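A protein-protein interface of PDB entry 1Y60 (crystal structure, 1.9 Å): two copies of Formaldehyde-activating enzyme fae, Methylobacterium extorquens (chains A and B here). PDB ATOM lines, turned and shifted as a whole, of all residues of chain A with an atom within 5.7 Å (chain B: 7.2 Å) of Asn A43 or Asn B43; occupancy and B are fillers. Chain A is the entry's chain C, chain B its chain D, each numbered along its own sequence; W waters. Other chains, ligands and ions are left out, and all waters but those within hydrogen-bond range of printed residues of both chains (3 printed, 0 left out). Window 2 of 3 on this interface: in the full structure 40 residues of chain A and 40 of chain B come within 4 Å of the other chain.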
ATOM      1  N   CYS A  38     -25.629 -25.782 -12.659  1.00  0.00           N
ATOM      2  CA  CYS A  38     -26.503 -24.682 -13.076  1.00  0.00           C
ATOM      3  C   CYS A  38     -26.189 -24.160 -14.478  1.00  0.00           C
ATOM      4  O   CYS A  38     -27.110 -23.891 -15.248  1.00  0.00           O
ATOM      5  CB  CYS A  38     -26.445 -23.507 -12.078  1.00  0.00           C
ATOM      6  SG  CYS A  38     -26.999 -23.861 -10.385  1.00  0.00           S
ATOM      7  N   ASN A  39     -24.904 -24.000 -14.802  1.00  0.00           N
ATOM      8  CA  ASN A  39     -24.503 -23.514 -16.124  1.00  0.00           C
ATOM      9  C   ASN A  39     -24.858 -24.559 -17.191  1.00  0.00           C
ATOM     10  O   ASN A  39     -25.152 -24.216 -18.345  1.00  0.00           O
ATOM     11  CB  ASN A  39     -22.980 -23.231 -16.185  1.00  0.00           C
ATOM     12  CG  ASN A  39     -22.554 -21.989 -15.371  1.00  0.00           C
ATOM     13  OD1 ASN A  39     -23.377 -21.183 -14.972  1.00  0.00           O
ATOM     14  ND2 ASN A  39     -21.249 -21.838 -15.149  1.00  0.00           N
ATOM     15  N   GLY A  40     -24.824 -25.832 -16.797  1.00  0.00           N
ATOM     16  CA  GLY A  40     -25.130 -26.918 -17.723  1.00  0.00           C
ATOM     17  C   GLY A  40     -26.599 -27.020 -18.060  1.00  0.00           C
ATOM     18  O   GLY A  40     -26.965 -27.171 -19.227  1.00  0.00           O
ATOM     19  N   LEU A  41     -27.459 -26.933 -17.051  1.00  0.00           N
ATOM     20  CA  LEU A  41     -28.912 -27.037 -17.297  1.00  0.00           C
ATOM     21  C   LEU A  41     -29.479 -25.979 -18.228  1.00  0.00           C
ATOM     22  O   LEU A  41     -30.318 -26.296 -19.061  1.00  0.00           O
ATOM     23  CB  LEU A  41     -29.700 -26.969 -15.990  1.00  0.00           C
ATOM     24  CG  LEU A  41     -31.194 -27.312 -16.062  1.00  0.00           C
ATOM     25  CD1 LEU A  41     -31.391 -28.752 -16.485  1.00  0.00           C
ATOM     26  CD2 LEU A  41     -31.823 -27.100 -14.695  1.00  0.00           C
ATOM     27  N   VAL A  42     -29.030 -24.730 -18.091  1.00  0.00           N
ATOM     28  CA  VAL A  42     -29.558 -23.649 -18.918  1.00  0.00           C
ATOM     29  C   VAL A  42     -29.053 -23.594 -20.350  1.00  0.00           C
ATOM     30  O   VAL A  42     -29.622 -22.885 -21.166  1.00  0.00           O
ATOM     31  CB  VAL A  42     -29.276 -22.227 -18.318  1.00  0.00           C
ATOM     32  CG1 VAL A  42     -29.771 -22.122 -16.873  1.00  0.00           C
ATOM     33  CG2 VAL A  42     -27.791 -21.893 -18.416  1.00  0.00           C
ATOM     34  N   ASN A  43     -28.006 -24.354 -20.649  1.00  0.00           N
ATOM     35  CA  ASN A  43     -27.377 -24.321 -21.965  1.00  0.00           C
ATOM     36  C   ASN A  43     -27.559 -25.553 -22.852  1.00  0.00           C
ATOM     37  O   ASN A  43     -26.776 -26.504 -22.787  1.00  0.00           O
ATOM     38  CB  ASN A  43     -25.884 -24.042 -21.760  1.00  0.00           C
ATOM     39  CG  ASN A  43     -25.126 -23.811 -23.060  1.00  0.00           C
ATOM     40  OD1 ASN A  43     -23.974 -24.165 -23.188  1.00  0.00           O
ATOM     41  ND2 ASN A  43     -25.754 -23.207 -23.994  1.00  0.00           N
ATOM     42  N   ASN A  44     -28.595 -25.520 -23.683  1.00  0.00           N
ATOM     43  CA  ASN A  44     -28.863 -26.610 -24.618  1.00  0.00           C
ATOM     44  C   ASN A  44     -28.492 -26.160 -26.019  1.00  0.00           C
ATOM     45  O   ASN A  44     -28.515 -24.963 -26.330  1.00  0.00           O
ATOM     46  CB  ASN A  44     -30.346 -27.011 -24.581  1.00  0.00           C
ATOM     47  CG  ASN A  44     -30.742 -27.579 -23.258  1.00  0.00           C
ATOM     48  OD1 ASN A  44     -29.972 -28.286 -22.627  1.00  0.00           O
ATOM     49  ND2 ASN A  44     -31.944 -27.285 -22.825  1.00  0.00           N
ATOM     50  N   LYS A  45     -28.114 -27.123 -26.847  1.00  0.00           N
ATOM     51  CA  LYS A  45     -27.747 -26.848 -28.227  1.00  0.00           C
ATOM     52  C   LYS A  45     -28.288 -27.987 -29.089  1.00  0.00           C
ATOM     53  O   LYS A  45     -28.721 -29.016 -28.564  1.00  0.00           O
ATOM     54  CB  LYS A  45     -26.219 -26.712 -28.395  1.00  0.00           C
ATOM     55  CG  LYS A  45     -25.372 -27.459 -27.411  1.00  0.00           C
ATOM     56  CD  LYS A  45     -24.819 -26.565 -26.325  1.00  0.00           C
ATOM     57  CE  LYS A  45     -25.045 -27.213 -24.956  1.00  0.00           C
ATOM     58  NZ  LYS A  45     -24.123 -28.330 -24.557  1.00  0.00           N
ATOM     59  N   PHE A  48     -27.649 -31.720 -28.410  1.00  0.00           N
ATOM     60  CA  PHE A  48     -27.210 -31.856 -27.028  1.00  0.00           C
ATOM     61  C   PHE A  48     -28.038 -31.071 -26.022  1.00  0.00           C
ATOM     62  O   PHE A  48     -27.798 -29.884 -25.777  1.00  0.00           O
ATOM     63  CB  PHE A  48     -25.747 -31.423 -26.901  1.00  0.00           C
ATOM     64  CG  PHE A  48     -24.798 -32.281 -27.673  1.00  0.00           C
ATOM     65  CD1 PHE A  48     -24.603 -32.070 -29.034  1.00  0.00           C
ATOM     66  CD2 PHE A  48     -24.151 -33.338 -27.056  1.00  0.00           C
ATOM     67  CE1 PHE A  48     -23.784 -32.908 -29.782  1.00  0.00           C
ATOM     68  CE2 PHE A  48     -23.325 -34.187 -27.781  1.00  0.00           C
ATOM     69  CZ  PHE A  48     -23.142 -33.972 -29.163  1.00  0.00           C
ATOM     70  N   SER A  50     -29.342 -31.024 -22.049  1.00  0.00           N
ATOM     71  CA  SER A  50     -29.034 -31.609 -20.757  1.00  0.00           C
ATOM     72  C   SER A  50     -30.283 -31.541 -19.893  1.00  0.00           C
ATOM     73  O   SER A  50     -30.986 -30.528 -19.888  1.00  0.00           O
ATOM     74  CB  SER A  50     -27.890 -30.830 -20.089  1.00  0.00           C
ATOM     75  OG  SER A  50     -26.747 -30.765 -20.938  1.00  0.00           O
ATOM     76  N   PHE A  68     -25.982 -35.394 -19.427  1.00  0.00           N
ATOM     77  CA  PHE A  68     -25.685 -34.821 -20.731  1.00  0.00           C
ATOM     78  C   PHE A  68     -25.157 -35.933 -21.639  1.00  0.00           C
ATOM     79  O   PHE A  68     -24.491 -36.854 -21.176  1.00  0.00           O
ATOM     80  CB  PHE A  68     -24.677 -33.660 -20.622  1.00  0.00           C
ATOM     81  CG  PHE A  68     -23.534 -33.915 -19.668  1.00  0.00           C
ATOM     82  CD1 PHE A  68     -22.284 -34.309 -20.139  1.00  0.00           C
ATOM     83  CD2 PHE A  68     -23.710 -33.767 -18.295  1.00  0.00           C
ATOM     84  CE1 PHE A  68     -21.226 -34.552 -19.264  1.00  0.00           C
ATOM     85  CE2 PHE A  68     -22.660 -34.010 -17.416  1.00  0.00           C
ATOM     86  CZ  PHE A  68     -21.408 -34.406 -17.902  1.00  0.00           C
ATOM     87  N   CYS B  38     -14.953 -28.579 -15.039  1.00  0.00           N
ATOM     88  CA  CYS B  38     -16.354 -28.948 -14.817  1.00  0.00           C
ATOM     89  C   CYS B  38     -17.297 -28.382 -15.879  1.00  0.00           C
ATOM     90  O   CYS B  38     -18.149 -29.113 -16.413  1.00  0.00           O
ATOM     91  CB  CYS B  38     -16.823 -28.500 -13.430  1.00  0.00           C
ATOM     92  SG  CYS B  38     -15.966 -29.258 -11.994  1.00  0.00           S
ATOM     93  N   ASN B  39     -17.126 -27.100 -16.208  1.00  0.00           N
ATOM     94  CA  ASN B  39     -17.961 -26.440 -17.218  1.00  0.00           C
ATOM     95  C   ASN B  39     -17.716 -27.065 -18.586  1.00  0.00           C
ATOM     96  O   ASN B  39     -18.628 -27.116 -19.424  1.00  0.00           O
ATOM     97  CB  ASN B  39     -17.648 -24.930 -17.319  1.00  0.00           C
ATOM     98  CG  ASN B  39     -18.195 -24.102 -16.128  1.00  0.00           C
ATOM     99  OD1 ASN B  39     -19.133 -24.499 -15.440  1.00  0.00           O
ATOM    100  ND2 ASN B  39     -17.613 -22.930 -15.920  1.00  0.00           N
ATOM    101  N   GLY B  40     -16.476 -27.508 -18.815  1.00  0.00           N
ATOM    102  CA  GLY B  40     -16.130 -28.148 -20.073  1.00  0.00           C
ATOM    103  C   GLY B  40     -16.720 -29.532 -20.267  1.00  0.00           C
ATOM    104  O   GLY B  40     -17.249 -29.833 -21.330  1.00  0.00           O
ATOM    105  N   LEU B  41     -16.626 -30.400 -19.257  1.00  0.00           N
ATOM    106  CA  LEU B  41     -17.163 -31.761 -19.387  1.00  0.00           C
ATOM    107  C   LEU B  41     -18.665 -31.813 -19.684  1.00  0.00           C
ATOM    108  O   LEU B  41     -19.101 -32.604 -20.509  1.00  0.00           O
ATOM    109  CB  LEU B  41     -16.908 -32.564 -18.121  1.00  0.00           C
ATOM    110  CG  LEU B  41     -17.231 -34.063 -18.224  1.00  0.00           C
ATOM    111  CD1 LEU B  41     -16.204 -34.734 -19.134  1.00  0.00           C
ATOM    112  CD2 LEU B  41     -17.183 -34.715 -16.858  1.00  0.00           C
ATOM    113  N   VAL B  42     -19.455 -30.969 -19.026  1.00  0.00           N
ATOM    114  CA  VAL B  42     -20.910 -30.984 -19.218  1.00  0.00           C
ATOM    115  C   VAL B  42     -21.424 -30.401 -20.523  1.00  0.00           C
ATOM    116  O   VAL B  42     -22.578 -30.620 -20.882  1.00  0.00           O
ATOM    117  CB  VAL B  42     -21.670 -30.204 -18.083  1.00  0.00           C
ATOM    118  CG1 VAL B  42     -21.185 -30.613 -16.703  1.00  0.00           C
ATOM    119  CG2 VAL B  42     -21.501 -28.701 -18.265  1.00  0.00           C
ATOM    120  N   ASN B  43     -20.574 -29.666 -21.231  1.00  0.00           N
ATOM    121  CA  ASN B  43     -20.977 -28.977 -22.455  1.00  0.00           C
ATOM    122  C   ASN B  43     -20.439 -29.526 -23.768  1.00  0.00           C
ATOM    123  O   ASN B  43     -19.349 -29.163 -24.203  1.00  0.00           O
ATOM    124  CB  ASN B  43     -20.602 -27.499 -22.301  1.00  0.00           C
ATOM    125  CG  ASN B  43     -20.956 -26.675 -23.501  1.00  0.00           C
ATOM    126  OD1 ASN B  43     -21.872 -26.989 -24.249  1.00  0.00           O
ATOM    127  ND2 ASN B  43     -20.228 -25.604 -23.693  1.00  0.00           N
ATOM    128  N   ASN B  44     -21.217 -30.396 -24.400  1.00  0.00           N
ATOM    129  CA  ASN B  44     -20.831 -30.996 -25.674  1.00  0.00           C
ATOM    130  C   ASN B  44     -21.671 -30.390 -26.792  1.00  0.00           C
ATOM    131  O   ASN B  44     -22.804 -29.967 -26.563  1.00  0.00           O
ATOM    132  CB  ASN B  44     -21.022 -32.518 -25.634  1.00  0.00           C
ATOM    133  CG  ASN B  44     -20.047 -33.194 -24.694  1.00  0.00           C
ATOM    134  OD1 ASN B  44     -18.909 -32.781 -24.574  1.00  0.00           O
ATOM    135  ND2 ASN B  44     -20.481 -34.242 -24.041  1.00  0.00           N
ATOM    136  N   LYS B  45     -21.096 -30.339 -27.992  1.00  0.00           N
ATOM    137  CA  LYS B  45     -21.766 -29.775 -29.143  1.00  0.00           C
ATOM    138  C   LYS B  45     -21.463 -30.659 -30.355  1.00  0.00           C
ATOM    139  O   LYS B  45     -20.563 -31.495 -30.316  1.00  0.00           O
ATOM    140  CB  LYS B  45     -21.255 -28.353 -29.408  1.00  0.00           C
ATOM    141  CG  LYS B  45     -21.249 -27.428 -28.192  1.00  0.00           C
ATOM    142  CD  LYS B  45     -19.890 -26.823 -27.860  1.00  0.00           C
ATOM    143  CE  LYS B  45     -19.085 -27.697 -26.910  1.00  0.00           C
ATOM    144  NZ  LYS B  45     -17.688 -27.202 -26.744  1.00  0.00           N
ATOM    145  N   PHE B  48     -17.885 -31.487 -31.423  1.00  0.00           N
ATOM    146  CA  PHE B  48     -16.995 -31.196 -30.317  1.00  0.00           C
ATOM    147  C   PHE B  48     -17.490 -31.758 -29.004  1.00  0.00           C
ATOM    148  O   PHE B  48     -18.311 -31.149 -28.328  1.00  0.00           O
ATOM    149  CB  PHE B  48     -16.818 -29.681 -30.167  1.00  0.00           C
ATOM    150  CG  PHE B  48     -16.119 -29.033 -31.316  1.00  0.00           C
ATOM    151  CD1 PHE B  48     -16.821 -28.701 -32.471  1.00  0.00           C
ATOM    152  CD2 PHE B  48     -14.744 -28.805 -31.271  1.00  0.00           C
ATOM    153  CE1 PHE B  48     -16.165 -28.156 -33.569  1.00  0.00           C
ATOM    154  CE2 PHE B  48     -14.078 -28.261 -32.362  1.00  0.00           C
ATOM    155  CZ  PHE B  48     -14.791 -27.938 -33.515  1.00  0.00           C
ATOM    156  N   THR B  49     -16.995 -32.930 -28.644  1.00  0.00           N
ATOM    157  CA  THR B  49     -17.390 -33.570 -27.395  1.00  0.00           C
ATOM    158  C   THR B  49     -16.120 -33.659 -26.581  1.00  0.00           C
ATOM    159  O   THR B  49     -15.077 -34.020 -27.096  1.00  0.00           O
ATOM    160  CB  THR B  49     -18.009 -34.982 -27.645  1.00  0.00           C
ATOM    161  OG1 THR B  49     -19.375 -34.832 -28.088  1.00  0.00           O
ATOM    162  CG2 THR B  49     -17.976 -35.826 -26.373  1.00  0.00           C
ATOM    163  N   SER B  50     -16.198 -33.269 -25.321  1.00  0.00           N
ATOM    164  CA  SER B  50     -15.037 -33.293 -24.449  1.00  0.00           C
ATOM    165  C   SER B  50     -15.151 -34.516 -23.549  1.00  0.00           C
ATOM    166  O   SER B  50     -16.237 -34.835 -23.061  1.00  0.00           O
ATOM    167  CB  SER B  50     -15.006 -32.023 -23.578  1.00  0.00           C
ATOM    168  OG  SER B  50     -14.897 -30.834 -24.349  1.00  0.00           O
HETATM  169  O   HOH W   1     -24.685 -29.231 -19.567  1.00  0.00           O
HETATM  170  O   HOH W   2     -23.621 -30.814 -23.181  1.00  0.00           O
HETATM  171  O   HOH W   3     -21.447 -22.730 -24.771  1.00  0.00           O
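Asn A43 touches Asn B43.
Asn B44 touches Phe A48.
Phe A48 touches Lys B45 (CE1 to C, 3.3 Å).
O of Leu B41 touches CE1 of Phe A68, 3.1 Å away.
CE1 of Phe A68 touches CA of Val B42 (3.6 Å).
Hydrophobic or aromatic side chains of chain A that line the printed part of chain B: Phe A48 and Phe A68.
Among the printed residues, no Asp or Glu carboxylate lies within 4 Å of a Lys or Arg side-chain nitrogen of the other chain.
Gly A40 touches none of the printed residues of chain B.
Val A42 touches none of the printed residues of chain B.
Of chain B, only Asn B43 comes within 4 Å of Asn A43.
Of the printed residues of chain B, Lys A45 touches Asn B43 (2.6 Å) and Asn B44 (2.9 Å).
Of the printed residues of chain B, Phe A48 touches Asn B44 and Lys B45.
Of the printed residues of chain A, Leu B41 touches Phe A68.
Asn B43 touches just these residues of chain A: Asn A43 (3.7 Å) and Lys A45 (2.6 Å).
Printed residues of chain A within 4 Å of Asn B44: Lys A45 (2.9 Å) and Phe A48 (3.3 Å).
Printed residues of chain A within 4 Å of Lys B45: Phe A48 (3.3 Å).
The side-chain amide oxygen of Asn B44 lies within hydrogen-bond range of the backbone NH of Ser B50 (2.9 Å).
Water W2 lies within hydrogen-bond range of O of Val B42, N of Asn B44 and NZ of Lys A45.
Water W1 lies within hydrogen-bond range of the backbone carbonyl oxygen of Val B42 (2.8 Å), the side-chain hydroxyl of Ser A50 (2.9 Å) and the backbone carbonyl oxygen of Gly A40 (3.1 Å).
Water W3 lies within hydrogen-bond range of ND2 of Asn B43 (3.3 Å) and OD1 of Asn A43 (3.3 Å).
Asn A43 touches its own counterpart, Asn B43.
Lys A45 touches Asn B43, but with the chains exchanged Asn A43 does not touch Lys B45 (6.6 Å).
Lys A45 touches Asn B44, but with the chains exchanged Asn A44 does not touch Lys B45 (7.7 Å).
Phe A48 touches Asn B44, but with the chains exchanged Asn A44 does not touch Phe B48 (11.6 Å).
ND2 of Asn A39 lies within hydrogen-bond range of OD1 of Asn B39 (3.4 Å).
OD1 of Asn B43 lies within hydrogen-bond range of NZ of Lys A45 (2.6 Å).
NZ of Lys A45 is in hydrogen-bond range of O of Asn B44.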
